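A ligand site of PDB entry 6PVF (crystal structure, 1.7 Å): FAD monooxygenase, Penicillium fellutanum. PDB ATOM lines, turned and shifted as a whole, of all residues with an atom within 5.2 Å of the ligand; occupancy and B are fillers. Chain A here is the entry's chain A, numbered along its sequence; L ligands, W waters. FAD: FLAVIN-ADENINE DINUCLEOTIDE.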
ATOM      1  N   VAL A  13     -27.885   7.154   7.472  1.00  0.00           N
ATOM      2  CA  VAL A  13     -28.355   5.841   7.065  1.00  0.00           C
ATOM      3  C   VAL A  13     -27.205   5.138   6.340  1.00  0.00           C
ATOM      4  O   VAL A  13     -26.875   5.476   5.193  1.00  0.00           O
ATOM      5  CB  VAL A  13     -29.610   5.915   6.190  1.00  0.00           C
ATOM      6  CG1 VAL A  13     -30.069   4.509   5.826  1.00  0.00           C
ATOM      7  CG2 VAL A  13     -30.709   6.679   6.915  1.00  0.00           C
ATOM      8  N   GLY A  14     -26.594   4.183   7.033  1.00  0.00           N
ATOM      9  CA  GLY A  14     -25.518   3.385   6.478  1.00  0.00           C
ATOM     10  C   GLY A  14     -24.163   3.835   6.994  1.00  0.00           C
ATOM     11  O   GLY A  14     -23.809   5.019   6.900  1.00  0.00           O
ATOM     12  N   LEU A  15     -23.411   2.892   7.542  1.00  0.00           N
ATOM     13  CA  LEU A  15     -22.081   3.154   8.072  1.00  0.00           C
ATOM     14  C   LEU A  15     -21.041   2.339   7.295  1.00  0.00           C
ATOM     15  O   LEU A  15     -20.293   1.549   7.879  1.00  0.00           O
ATOM     16  CB  LEU A  15     -22.030   2.863   9.572  1.00  0.00           C
ATOM     17  CG  LEU A  15     -22.728   3.942  10.404  1.00  0.00           C
ATOM     18  CD1 LEU A  15     -22.768   3.536  11.883  1.00  0.00           C
ATOM     19  CD2 LEU A  15     -22.091   5.326  10.234  1.00  0.00           C
ATOM     20  N   GLY A  16     -21.019   2.517   5.981  1.00  0.00           N
ATOM     21  CA  GLY A  16     -19.817   2.201   5.229  1.00  0.00           C
ATOM     22  C   GLY A  16     -18.772   3.283   5.450  1.00  0.00           C
ATOM     23  O   GLY A  16     -18.852   4.046   6.421  1.00  0.00           O
ATOM     24  N   ILE A  17     -17.783   3.381   4.561  1.00  0.00           N
ATOM     25  CA  ILE A  17     -16.750   4.394   4.744  1.00  0.00           C
ATOM     26  C   ILE A  17     -17.347   5.796   4.762  1.00  0.00           C
ATOM     27  O   ILE A  17     -16.948   6.640   5.567  1.00  0.00           O
ATOM     28  CB  ILE A  17     -15.676   4.249   3.653  1.00  0.00           C
ATOM     29  CG1 ILE A  17     -15.028   2.870   3.747  1.00  0.00           C
ATOM     30  CG2 ILE A  17     -14.627   5.379   3.743  1.00  0.00           C
ATOM     31  CD1 ILE A  17     -14.309   2.472   2.469  1.00  0.00           C
ATOM     32  N   VAL A  18     -18.312   6.061   3.872  1.00  0.00           N
ATOM     33  CA  VAL A  18     -18.817   7.433   3.713  1.00  0.00           C
ATOM     34  C   VAL A  18     -19.715   7.831   4.885  1.00  0.00           C
ATOM     35  O   VAL A  18     -19.645   8.976   5.371  1.00  0.00           O
ATOM     36  CB  VAL A  18     -19.555   7.567   2.374  1.00  0.00           C
ATOM     37  CG1 VAL A  18     -20.123   8.982   2.222  1.00  0.00           C
ATOM     38  CG2 VAL A  18     -18.596   7.230   1.233  1.00  0.00           C
ATOM     39  N   GLY A  19     -20.572   6.919   5.346  1.00  0.00           N
ATOM     40  CA  GLY A  19     -21.395   7.222   6.492  1.00  0.00           C
ATOM     41  C   GLY A  19     -20.575   7.457   7.736  1.00  0.00           C
ATOM     42  O   GLY A  19     -20.891   8.342   8.536  1.00  0.00           O
ATOM     43  N   PHE A  36     -27.310   4.870  11.757  1.00  0.00           N
ATOM     44  CA  PHE A  36     -27.974   3.579  11.733  1.00  0.00           C
ATOM     45  C   PHE A  36     -27.315   2.687  10.695  1.00  0.00           C
ATOM     46  O   PHE A  36     -26.941   3.170   9.626  1.00  0.00           O
ATOM     47  CB  PHE A  36     -29.456   3.755  11.408  1.00  0.00           C
ATOM     48  CG  PHE A  36     -30.198   4.529  12.446  1.00  0.00           C
ATOM     49  CD1 PHE A  36     -30.756   3.877  13.533  1.00  0.00           C
ATOM     50  CD2 PHE A  36     -30.307   5.911  12.361  1.00  0.00           C
ATOM     51  CE1 PHE A  36     -31.417   4.585  14.515  1.00  0.00           C
ATOM     52  CE2 PHE A  36     -30.987   6.622  13.343  1.00  0.00           C
ATOM     53  CZ  PHE A  36     -31.547   5.960  14.419  1.00  0.00           C
ATOM     54  N   GLU A  37     -27.207   1.401  10.998  1.00  0.00           N
ATOM     55  CA  GLU A  37     -26.537   0.480  10.091  1.00  0.00           C
ATOM     56  C   GLU A  37     -27.136  -0.912  10.283  1.00  0.00           C
ATOM     57  O   GLU A  37     -27.333  -1.356  11.407  1.00  0.00           O
ATOM     58  CB  GLU A  37     -25.014   0.467  10.364  1.00  0.00           C
ATOM     59  CG  GLU A  37     -24.273  -0.756   9.847  1.00  0.00           C
ATOM     60  CD  GLU A  37     -24.266  -0.873   8.328  1.00  0.00           C
ATOM     61  OE1 GLU A  37     -23.924   0.131   7.667  1.00  0.00           O
ATOM     62  OE2 GLU A  37     -24.542  -1.980   7.814  1.00  0.00           O
ATOM     63  N   LYS A  38     -27.431  -1.588   9.167  1.00  0.00           N
ATOM     64  CA  LYS A  38     -28.149  -2.856   9.311  1.00  0.00           C
ATOM     65  C   LYS A  38     -27.250  -4.033   9.689  1.00  0.00           C
ATOM     66  O   LYS A  38     -27.757  -5.019  10.214  1.00  0.00           O
ATOM     67  CB  LYS A  38     -28.902  -3.186   8.012  1.00  0.00           C
ATOM     68  CG  LYS A  38     -28.002  -3.412   6.827  1.00  0.00           C
ATOM     69  CD  LYS A  38     -28.826  -3.728   5.574  1.00  0.00           C
ATOM     70  CE  LYS A  38     -27.914  -4.098   4.413  1.00  0.00           C
ATOM     71  NZ  LYS A  38     -28.665  -4.245   3.140  1.00  0.00           N
ATOM     72  N   SER A  39     -25.934  -3.954   9.442  1.00  0.00           N
ATOM     73  CA  SER A  39     -25.051  -5.102   9.578  1.00  0.00           C
ATOM     74  C   SER A  39     -23.994  -4.882  10.651  1.00  0.00           C
ATOM     75  O   SER A  39     -23.742  -3.752  11.084  1.00  0.00           O
ATOM     76  CB  SER A  39     -24.344  -5.406   8.248  1.00  0.00           C
ATOM     77  OG  SER A  39     -25.279  -5.829   7.275  1.00  0.00           O
ATOM     78  N   ILE A  41     -20.708  -4.173  10.877  1.00  0.00           N
ATOM     79  CA  ILE A  41     -19.717  -3.629   9.948  1.00  0.00           C
ATOM     80  C   ILE A  41     -18.292  -3.926  10.364  1.00  0.00           C
ATOM     81  O   ILE A  41     -17.364  -3.570   9.627  1.00  0.00           O
ATOM     82  CB  ILE A  41     -19.847  -2.102   9.779  1.00  0.00           C
ATOM     83  CG1 ILE A  41     -19.903  -1.399  11.142  1.00  0.00           C
ATOM     84  CG2 ILE A  41     -21.078  -1.777   8.949  1.00  0.00           C
ATOM     85  CD1 ILE A  41     -19.905   0.116  11.038  1.00  0.00           C
ATOM     86  N   ILE A  45     -14.512  -8.624   5.756  1.00  0.00           N
ATOM     87  CA  ILE A  45     -15.067  -8.879   4.432  1.00  0.00           C
ATOM     88  C   ILE A  45     -14.432  -7.893   3.460  1.00  0.00           C
ATOM     89  O   ILE A  45     -14.023  -6.803   3.860  1.00  0.00           O
ATOM     90  CB  ILE A  45     -16.613  -8.756   4.456  1.00  0.00           C
ATOM     91  CG1 ILE A  45     -17.212  -9.145   3.103  1.00  0.00           C
ATOM     92  CG2 ILE A  45     -17.019  -7.342   4.850  1.00  0.00           C
ATOM     93  CD1 ILE A  45     -18.709  -9.204   3.123  1.00  0.00           C
ATOM     94  N   GLY A  46     -14.296  -8.305   2.193  1.00  0.00           N
ATOM     95  CA  GLY A  46     -13.702  -7.444   1.183  1.00  0.00           C
ATOM     96  C   GLY A  46     -12.179  -7.511   1.217  1.00  0.00           C
ATOM     97  O   GLY A  46     -11.585  -8.342   1.907  1.00  0.00           O
ATOM     98  N   ASP A  47     -11.548  -6.613   0.478  1.00  0.00           N
ATOM     99  CA  ASP A  47     -10.090  -6.586   0.517  1.00  0.00           C
ATOM    100  C   ASP A  47      -9.592  -5.187   0.883  1.00  0.00           C
ATOM    101  O   ASP A  47      -9.968  -4.683   1.950  1.00  0.00           O
ATOM    102  CB  ASP A  47      -9.461  -7.151  -0.790  1.00  0.00           C
ATOM    103  CG  ASP A  47      -9.920  -6.425  -2.053  1.00  0.00           C
ATOM    104  OD1 ASP A  47      -9.265  -5.434  -2.453  1.00  0.00           O
ATOM    105  OD2 ASP A  47     -10.887  -6.888  -2.686  1.00  0.00           O
ATOM    106  N   CYS A  48      -8.781  -4.547   0.056  1.00  0.00           N
ATOM    107  CA  CYS A  48      -8.138  -3.297   0.430  1.00  0.00           C
ATOM    108  C   CYS A  48      -8.817  -2.083  -0.192  1.00  0.00           C
ATOM    109  O   CYS A  48      -9.355  -2.144  -1.300  1.00  0.00           O
ATOM    110  CB  CYS A  48      -6.654  -3.272   0.050  1.00  0.00           C
ATOM    111  SG  CYS A  48      -5.593  -4.119   1.226  1.00  0.00           S
ATOM    112  N   ILE A  49      -8.797  -0.986   0.555  1.00  0.00           N
ATOM    113  CA  ILE A  49      -9.305   0.310   0.118  1.00  0.00           C
ATOM    114  C   ILE A  49      -8.129   1.261   0.016  1.00  0.00           C
ATOM    115  O   ILE A  49      -7.262   1.289   0.896  1.00  0.00           O
ATOM    116  CB  ILE A  49     -10.352   0.856   1.120  1.00  0.00           C
ATOM    117  CG1 ILE A  49     -11.700   0.175   0.899  1.00  0.00           C
ATOM    118  CG2 ILE A  49     -10.504   2.376   0.970  1.00  0.00           C
ATOM    119  CD1 ILE A  49     -12.525   0.828  -0.185  1.00  0.00           C
ATOM    120  N   ARG A 109     -10.310  -2.858   3.978  1.00  0.00           N
ATOM    121  CA  ARG A 109     -11.512  -2.082   4.280  1.00  0.00           C
ATOM    122  C   ARG A 109     -11.951  -2.283   5.720  1.00  0.00           C
ATOM    123  O   ARG A 109     -12.307  -1.311   6.407  1.00  0.00           O
ATOM    124  CB  ARG A 109     -12.644  -2.459   3.329  1.00  0.00           C
ATOM    125  CG  ARG A 109     -13.919  -1.610   3.516  1.00  0.00           C
ATOM    126  CD  ARG A 109     -14.988  -2.090   2.549  1.00  0.00           C
ATOM    127  NE  ARG A 109     -16.250  -1.347   2.659  1.00  0.00           N
ATOM    128  CZ  ARG A 109     -17.189  -1.616   3.564  1.00  0.00           C
ATOM    129  NH1 ARG A 109     -16.995  -2.594   4.443  1.00  0.00           N
ATOM    130  NH2 ARG A 109     -18.321  -0.908   3.599  1.00  0.00           N
ATOM    131  N   VAL A 131     -30.013  -2.195  12.535  1.00  0.00           N
ATOM    132  CA  VAL A 131     -31.189  -1.415  12.177  1.00  0.00           C
ATOM    133  C   VAL A 131     -31.232  -1.248  10.670  1.00  0.00           C
ATOM    134  O   VAL A 131     -30.335  -0.640  10.087  1.00  0.00           O
ATOM    135  CB  VAL A 131     -31.215  -0.036  12.845  1.00  0.00           C
ATOM    136  CG1 VAL A 131     -32.413   0.767  12.365  1.00  0.00           C
ATOM    137  CG2 VAL A 131     -31.242  -0.200  14.359  1.00  0.00           C
ATOM    138  N   GLU A 132     -32.317  -1.739  10.064  1.00  0.00           N
ATOM    139  CA  GLU A 132     -32.645  -1.437   8.674  1.00  0.00           C
ATOM    140  C   GLU A 132     -33.524  -0.187   8.656  1.00  0.00           C
ATOM    141  O   GLU A 132     -34.633  -0.187   9.198  1.00  0.00           O
ATOM    142  CB  GLU A 132     -33.376  -2.615   8.025  1.00  0.00           C
ATOM    143  CG  GLU A 132     -33.824  -2.362   6.593  1.00  0.00           C
ATOM    144  CD  GLU A 132     -34.607  -3.529   6.022  1.00  0.00           C
ATOM    145  OE1 GLU A 132     -34.655  -4.597   6.675  1.00  0.00           O
ATOM    146  OE2 GLU A 132     -35.188  -3.379   4.918  1.00  0.00           O
ATOM    147  N   VAL A 133     -33.029   0.881   8.028  1.00  0.00           N
ATOM    148  CA  VAL A 133     -33.772   2.125   7.914  1.00  0.00           C
ATOM    149  C   VAL A 133     -34.686   2.050   6.704  1.00  0.00           C
ATOM    150  O   VAL A 133     -34.256   1.668   5.616  1.00  0.00           O
ATOM    151  CB  VAL A 133     -32.842   3.345   7.809  1.00  0.00           C
ATOM    152  CG1 VAL A 133     -33.692   4.618   7.690  1.00  0.00           C
ATOM    153  CG2 VAL A 133     -31.926   3.429   9.009  1.00  0.00           C
ATOM    154  N   SER A 165     -26.292   7.450   3.166  1.00  0.00           N
ATOM    155  CA  SER A 165     -25.016   6.894   2.782  1.00  0.00           C
ATOM    156  C   SER A 165     -25.110   5.374   2.733  1.00  0.00           C
ATOM    157  O   SER A 165     -24.254   4.666   3.279  1.00  0.00           O
ATOM    158  CB  SER A 165     -23.916   7.378   3.760  1.00  0.00           C
ATOM    159  OG  SER A 165     -24.353   7.277   5.108  1.00  0.00           O
ATOM    160  N   ASP A 166     -26.157   4.855   2.069  1.00  0.00           N
ATOM    161  CA  ASP A 166     -26.462   3.438   2.160  1.00  0.00           C
ATOM    162  C   ASP A 166     -25.970   2.646   0.934  1.00  0.00           C
ATOM    163  O   ASP A 166     -26.431   1.527   0.703  1.00  0.00           O
ATOM    164  CB  ASP A 166     -27.965   3.232   2.434  1.00  0.00           C
ATOM    165  CG  ASP A 166     -28.880   3.975   1.465  1.00  0.00           C
ATOM    166  OD1 ASP A 166     -28.495   4.992   0.824  1.00  0.00           O
ATOM    167  OD2 ASP A 166     -30.063   3.561   1.413  1.00  0.00           O
ATOM    168  N   GLY A 167     -24.997   3.187   0.195  1.00  0.00           N
ATOM    169  CA  GLY A 167     -24.246   2.372  -0.752  1.00  0.00           C
ATOM    170  C   GLY A 167     -24.902   2.226  -2.112  1.00  0.00           C
ATOM    171  O   GLY A 167     -25.925   2.847  -2.442  1.00  0.00           O
ATOM    172  N   VAL A 168     -24.262   1.383  -2.942  1.00  0.00           N
ATOM    173  CA  VAL A 168     -24.649   1.309  -4.345  1.00  0.00           C
ATOM    174  C   VAL A 168     -26.066   0.764  -4.511  1.00  0.00           C
ATOM    175  O   VAL A 168     -26.759   1.110  -5.474  1.00  0.00           O
ATOM    176  CB  VAL A 168     -23.593   0.471  -5.120  1.00  0.00           C
ATOM    177  CG1 VAL A 168     -23.538  -0.944  -4.596  1.00  0.00           C
ATOM    178  CG2 VAL A 168     -23.911   0.475  -6.623  1.00  0.00           C
ATOM    179  N   ARG A 192     -10.542 -10.096  -7.145  1.00  0.00           N
ATOM    180  CA  ARG A 192      -9.748  -9.342  -6.184  1.00  0.00           C
ATOM    181  C   ARG A 192      -9.842 -10.014  -4.831  1.00  0.00           C
ATOM    182  O   ARG A 192     -10.861 -10.614  -4.492  1.00  0.00           O
ATOM    183  CB  ARG A 192     -10.192  -7.865  -6.093  1.00  0.00           C
ATOM    184  CG  ARG A 192     -11.675  -7.554  -6.261  1.00  0.00           C
ATOM    185  CD  ARG A 192     -11.944  -6.030  -6.285  1.00  0.00           C
ATOM    186  NE  ARG A 192     -11.300  -5.337  -5.157  1.00  0.00           N
ATOM    187  CZ  ARG A 192     -10.582  -4.220  -5.268  1.00  0.00           C
ATOM    188  NH1 ARG A 192     -10.430  -3.647  -6.457  1.00  0.00           N
ATOM    189  NH2 ARG A 192     -10.022  -3.665  -4.191  1.00  0.00           N
ATOM    190  N   TRP A 256     -20.183  -8.009  -2.589  1.00  0.00           N
ATOM    191  CA  TRP A 256     -18.873  -8.426  -2.134  1.00  0.00           C
ATOM    192  C   TRP A 256     -18.893  -9.773  -1.424  1.00  0.00           C
ATOM    193  O   TRP A 256     -17.935 -10.112  -0.723  1.00  0.00           O
ATOM    194  CB  TRP A 256     -18.271  -7.343  -1.228  1.00  0.00           C
ATOM    195  CG  TRP A 256     -17.991  -6.095  -1.997  1.00  0.00           C
ATOM    196  CD1 TRP A 256     -18.861  -5.063  -2.230  1.00  0.00           C
ATOM    197  CD2 TRP A 256     -16.784  -5.759  -2.684  1.00  0.00           C
ATOM    198  NE1 TRP A 256     -18.257  -4.100  -3.012  1.00  0.00           N
ATOM    199  CE2 TRP A 256     -16.977  -4.503  -3.289  1.00  0.00           C
ATOM    200  CE3 TRP A 256     -15.541  -6.387  -2.817  1.00  0.00           C
ATOM    201  CZ2 TRP A 256     -15.988  -3.874  -4.040  1.00  0.00           C
ATOM    202  CZ3 TRP A 256     -14.551  -5.748  -3.558  1.00  0.00           C
ATOM    203  CH2 TRP A 256     -14.787  -4.504  -4.165  1.00  0.00           C
ATOM    204  N   ILE A 314     -25.270  10.669  -0.595  1.00  0.00           N
ATOM    205  CA  ILE A 314     -23.829  10.837  -0.759  1.00  0.00           C
ATOM    206  C   ILE A 314     -23.178   9.474  -0.916  1.00  0.00           C
ATOM    207  O   ILE A 314     -23.806   8.424  -0.714  1.00  0.00           O
ATOM    208  CB  ILE A 314     -23.178  11.631   0.396  1.00  0.00           C
ATOM    209  CG1 ILE A 314     -23.309  10.863   1.710  1.00  0.00           C
ATOM    210  CG2 ILE A 314     -23.749  13.080   0.474  1.00  0.00           C
ATOM    211  CD1 ILE A 314     -22.522  11.510   2.863  1.00  0.00           C
ATOM    212  N   GLY A 315     -21.890   9.485  -1.273  1.00  0.00           N
ATOM    213  CA  GLY A 315     -21.180   8.222  -1.430  1.00  0.00           C
ATOM    214  C   GLY A 315     -21.677   7.430  -2.630  1.00  0.00           C
ATOM    215  O   GLY A 315     -22.112   8.002  -3.649  1.00  0.00           O
ATOM    216  N   ASP A 316     -21.641   6.103  -2.509  1.00  0.00           N
ATOM    217  CA  ASP A 316     -22.067   5.218  -3.594  1.00  0.00           C
ATOM    218  C   ASP A 316     -23.578   5.260  -3.797  1.00  0.00           C
ATOM    219  O   ASP A 316     -24.057   4.863  -4.865  1.00  0.00           O
ATOM    220  CB  ASP A 316     -21.643   3.761  -3.336  1.00  0.00           C
ATOM    221  CG  ASP A 316     -20.139   3.530  -3.580  1.00  0.00           C
ATOM    222  OD1 ASP A 316     -19.408   4.520  -3.827  1.00  0.00           O
ATOM    223  OD2 ASP A 316     -19.696   2.351  -3.548  1.00  0.00           O
ATOM    224  N   ALA A 317     -24.339   5.752  -2.813  1.00  0.00           N
ATOM    225  CA  ALA A 317     -25.761   5.990  -3.068  1.00  0.00           C
ATOM    226  C   ALA A 317     -25.968   7.079  -4.110  1.00  0.00           C
ATOM    227  O   ALA A 317     -26.953   7.045  -4.844  1.00  0.00           O
ATOM    228  CB  ALA A 317     -26.476   6.356  -1.769  1.00  0.00           C
ATOM    229  N   LEU A 321     -18.870   4.280  -8.117  1.00  0.00           N
ATOM    230  CA  LEU A 321     -17.714   4.134  -8.985  1.00  0.00           C
ATOM    231  C   LEU A 321     -17.178   2.715  -8.814  1.00  0.00           C
ATOM    232  O   LEU A 321     -17.210   2.160  -7.712  1.00  0.00           O
ATOM    233  CB  LEU A 321     -16.609   5.126  -8.629  1.00  0.00           C
ATOM    234  CG  LEU A 321     -16.320   6.360  -9.458  1.00  0.00           C
ATOM    235  CD1 LEU A 321     -17.196   7.495  -9.023  1.00  0.00           C
ATOM    236  CD2 LEU A 321     -14.862   6.695  -9.245  1.00  0.00           C
ATOM    237  N   PRO A 323     -14.563  -0.259  -8.217  1.00  0.00           N
ATOM    238  CA  PRO A 323     -13.316  -0.344  -7.451  1.00  0.00           C
ATOM    239  C   PRO A 323     -12.078  -0.272  -8.331  1.00  0.00           C
ATOM    240  O   PRO A 323     -10.975  -0.080  -7.797  1.00  0.00           O
ATOM    241  CB  PRO A 323     -13.419  -1.697  -6.744  1.00  0.00           C
ATOM    242  CG  PRO A 323     -14.355  -2.484  -7.599  1.00  0.00           C
ATOM    243  CD  PRO A 323     -15.374  -1.490  -8.077  1.00  0.00           C
ATOM    244  N   GLY A 328     -13.224   6.076  -5.602  1.00  0.00           N
ATOM    245  CA  GLY A 328     -14.541   5.840  -5.031  1.00  0.00           C
ATOM    246  C   GLY A 328     -14.720   6.273  -3.586  1.00  0.00           C
ATOM    247  O   GLY A 328     -15.613   7.073  -3.275  1.00  0.00           O
ATOM    248  N   ALA A 329     -13.875   5.745  -2.694  1.00  0.00           N
ATOM    249  CA  ALA A 329     -13.954   6.108  -1.284  1.00  0.00           C
ATOM    250  C   ALA A 329     -13.572   7.567  -1.074  1.00  0.00           C
ATOM    251  O   ALA A 329     -14.187   8.263  -0.260  1.00  0.00           O
ATOM    252  CB  ALA A 329     -13.043   5.201  -0.462  1.00  0.00           C
HETATM  253  PA  FAD L   1     -20.887   1.144   1.273  1.00  0.00           P
HETATM  254  O1A FAD L   1     -21.497   0.173   0.333  1.00  0.00           O
HETATM  255  O2A FAD L   1     -19.454   0.987   1.636  1.00  0.00           O
HETATM  256  O5B FAD L   1     -21.663   1.136   2.627  1.00  0.00           O
HETATM  257  C5B FAD L   1     -23.109   1.190   2.667  1.00  0.00           C
HETATM  258  C4B FAD L   1     -23.543   0.723   4.043  1.00  0.00           C
HETATM  259  O4B FAD L   1     -24.950   1.027   4.229  1.00  0.00           O
HETATM  260  C3B FAD L   1     -23.371  -0.768   4.333  1.00  0.00           C
HETATM  261  O3B FAD L   1     -22.670  -0.959   5.563  1.00  0.00           O
HETATM  262  C2B FAD L   1     -24.812  -1.295   4.366  1.00  0.00           C
HETATM  263  O2B FAD L   1     -24.985  -2.377   5.265  1.00  0.00           O
HETATM  264  C1B FAD L   1     -25.563  -0.070   4.873  1.00  0.00           C
HETATM  265  N9A FAD L   1     -26.987  -0.026   4.553  1.00  0.00           N
HETATM  266  C8A FAD L   1     -27.565  -0.214   3.326  1.00  0.00           C
HETATM  267  N7A FAD L   1     -28.872  -0.074   3.338  1.00  0.00           N
HETATM  268  C5A FAD L   1     -29.163   0.225   4.663  1.00  0.00           C
HETATM  269  C6A FAD L   1     -30.377   0.510   5.315  1.00  0.00           C
HETATM  270  N6A FAD L   1     -31.564   0.516   4.714  1.00  0.00           N
HETATM  271  N1A FAD L   1     -30.315   0.795   6.642  1.00  0.00           N
HETATM  272  C2A FAD L   1     -29.134   0.760   7.254  1.00  0.00           C
HETATM  273  N3A FAD L   1     -27.924   0.538   6.730  1.00  0.00           N
HETATM  274  C4A FAD L   1     -28.016   0.259   5.422  1.00  0.00           C
HETATM  275  N1  FAD L   1     -14.523  -1.317  -2.146  1.00  0.00           N
HETATM  276  C2  FAD L   1     -13.218  -1.542  -2.487  1.00  0.00           C
HETATM  277  O2  FAD L   1     -12.601  -0.773  -3.224  1.00  0.00           O
HETATM  278  N3  FAD L   1     -12.569  -2.661  -1.969  1.00  0.00           N
HETATM  279  C4  FAD L   1     -13.122  -3.613  -1.125  1.00  0.00           C
HETATM  280  O4  FAD L   1     -12.437  -4.567  -0.760  1.00  0.00           O
HETATM  281  C4X FAD L   1     -14.514  -3.360  -0.779  1.00  0.00           C
HETATM  282  N5  FAD L   1     -15.130  -4.220   0.020  1.00  0.00           N
HETATM  283  C5X FAD L   1     -16.446  -3.952   0.349  1.00  0.00           C
HETATM  284  C6  FAD L   1     -17.129  -4.829   1.197  1.00  0.00           C
HETATM  285  C7  FAD L   1     -18.453  -4.599   1.556  1.00  0.00           C
HETATM  286  C7M FAD L   1     -19.164  -5.561   2.475  1.00  0.00           C
HETATM  287  C8  FAD L   1     -19.120  -3.457   1.067  1.00  0.00           C
HETATM  288  C8M FAD L   1     -20.559  -3.185   1.422  1.00  0.00           C
HETATM  289  C9  FAD L   1     -18.448  -2.577   0.230  1.00  0.00           C
HETATM  290  C9A FAD L   1     -17.125  -2.817  -0.140  1.00  0.00           C
HETATM  291  N10 FAD L   1     -16.422  -1.944  -0.996  1.00  0.00           N
HETATM  292  C10 FAD L   1     -15.120  -2.179  -1.327  1.00  0.00           C
HETATM  293  C1' FAD L   1     -17.076  -0.744  -1.536  1.00  0.00           C
HETATM  294  C2' FAD L   1     -16.645   0.530  -0.840  1.00  0.00           C
HETATM  295  O2' FAD L   1     -16.974   0.471   0.551  1.00  0.00           O
HETATM  296  C3' FAD L   1     -17.336   1.725  -1.501  1.00  0.00           C
HETATM  297  O3' FAD L   1     -17.136   1.635  -2.903  1.00  0.00           O
HETATM  298  C4' FAD L   1     -16.857   3.099  -1.035  1.00  0.00           C
HETATM  299  O4' FAD L   1     -15.458   3.080  -0.717  1.00  0.00           O
HETATM  300  C5' FAD L   1     -17.678   3.635   0.115  1.00  0.00           C
HETATM  301  O5' FAD L   1     -19.068   3.631  -0.273  1.00  0.00           O
HETATM  302  P   FAD L   1     -20.211   3.940   0.762  1.00  0.00           P
HETATM  303  O1P FAD L   1     -21.018   5.054   0.099  1.00  0.00           O
HETATM  304  O2P FAD L   1     -19.738   4.150   2.175  1.00  0.00           O
HETATM  305  O3P FAD L   1     -21.093   2.617   0.702  1.00  0.00           O
HETATM  306  O   HOH W   1     -21.622   4.590   4.062  1.00  0.00           O
HETATM  307  O   HOH W   2     -21.431   0.575  -2.376  1.00  0.00           O
HETATM  308  O   HOH W   3     -30.833   1.123   1.572  1.00  0.00           O
HETATM  309  O   HOH W   4     -23.393  -1.678   0.030  1.00  0.00           O
HETATM  310  O   HOH W   5     -10.397  -0.292  -4.250  1.00  0.00           O
HETATM  311  O   HOH W   6     -20.034  -0.948   6.123  1.00  0.00           O
HETATM  312  O   HOH W   7     -23.976  -3.636   1.855  1.00  0.00           O
HETATM  313  O   HOH W   8     -14.152   1.449  -3.587  1.00  0.00           O
HETATM  314  O   HOH W   9     -23.605   5.817   0.103  1.00  0.00           O
HETATM  315  O   HOH W  10     -30.959  -2.380   2.388  1.00  0.00           O
HETATM  316  O   HOH W  11     -15.347   2.787  -5.550  1.00  0.00           O
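The backbone NH (N) of Lys 38 is in hydrogen-bond range of a nitrogen (N3A) of the ligand. O2B of the ligand lies within hydrogen-bond range of OE2 of Glu 37, at 2.6 Å. O1P of the ligand lies within hydrogen-bond range of N of Asp 316 (2.9 Å). The side-chain carboxylate of Asp 316 is in hydrogen-bond range of an oxygen (O3') of the ligand (2.7 Å). The backbone carbonyl oxygen (O) of Val 133 sits at hydrogen-bond distance from a nitrogen (N6A) of the ligand (3.1 Å). N3 of the ligand sits at hydrogen-bond distance from O of Cys 48 (3.3 Å). O2A of the ligand is in salt-bridge range of NH2 of Arg 109, 3.0 Å away. The backbone NH (N) of Val 18 lies within hydrogen-bond range of an oxygen (O2P) of the ligand (2.9 Å). The backbone NH (N) of Ile 17 lies within hydrogen-bond range of an oxygen (O2P) of the ligand (3.2 Å). The backbone NH of Val 133 sits at hydrogen-bond distance from a nitrogen (N1A) of the ligand, at 3.0 Å. An oxygen (O4) of the ligand is in hydrogen-bond range of the backbone NH (N) of Asp 47, at 2.6 Å.
O of Phe 36 sits at hydrogen-bond distance from N of Gly 14 (2.8 Å). N of Ser 39 is in hydrogen-bond range of OE2 of Glu 37, 2.9 Å away. The backbone carbonyl oxygen (O) of Glu 37 sits at hydrogen-bond distance from the backbone NH (N) of Val 131 (3.0 Å). The backbone NH (N) of Asp 166 lies within hydrogen-bond range of the backbone carbonyl oxygen (O) of Val 13. The backbone NH (N) of Arg 109 sits at hydrogen-bond distance from the backbone carbonyl oxygen (O) of Asp 47 (2.7 Å). The side-chain carboxylate of Asp 47 is in salt-bridge range of the guanidinium group of Arg 192 (2.6 Å). The backbone NH (N) of Lys 38 is in hydrogen-bond range of the backbone carbonyl oxygen (O) of Val 131. O of Gly 14 lies within hydrogen-bond range of OG of Ser 165, at 2.9 Å.
N10 of the ligand lies close to NE1 of Trp 256 (3.5 Å). Val 13 touches the ligand (CG1 to N1A, 3.8 Å). CA of Gly 14 touches O4B of the ligand, at 3.3 Å. CA of Gly 16 touches O5B of the ligand (3.4 Å). Ile 41 touches the ligand (CG2 to O3B, 3.8 Å). CG2 of Ile 45 touches C7M of the ligand, 3.7 Å away. C of Gly 46 touches O4 of the ligand, 3.6 Å away. Ile 49 touches the ligand (CD1 to C2, 3.4 Å). Val 131 touches the ligand (O to C2A, 3.4 Å). CA of Glu 132 touches N1A of the ligand (3.8 Å). O of Ser 165 touches C5B of the ligand, at 3.7 Å. O of Asp 166 touches C8A of the ligand, 3.3 Å away. Gly 167 touches the ligand (CA to O3P, 3.5 Å). Arg 192 touches the ligand (NH2 to N3, 3.5 Å). CA of Gly 315 touches O1P of the ligand (3.5 Å). Pro 323 touches the ligand (CB to O2, 3.7 Å). Ala 329 touches the ligand. Hydrophobic or aromatic side chains that line the ligand: Val 13, Ile 17, Val 18, Ile 41, Ile 45, Ile 49, Val 133, Trp 256, Pro 323 and Ala 329. The nearest printed residue that does not touch the ligand is Ser 39 (4.01 Å).
Water W5 bridges O2 of the ligand and NH2 of Arg 192. Water W6 lies within hydrogen-bond range of O3B of the ligand, NH2 of Arg 109 and O of Leu 15. Water W1 lies within hydrogen-bond range of O2P of the ligand, O of Ser 165, N of Gly 19 and N of Gly 16. Water W2 lies within hydrogen-bond range of O1A of the ligand, OD2 of Asp 316 and N of Val 168. Water W10 lies within hydrogen-bond range of the side-chain amino group (NZ) of Lys 38 and a nitrogen (N7A) of the ligand. Water W11 lies within hydrogen-bond range of O of Leu 321 (2.9 Å) and O3' of the ligand (3.4 Å).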
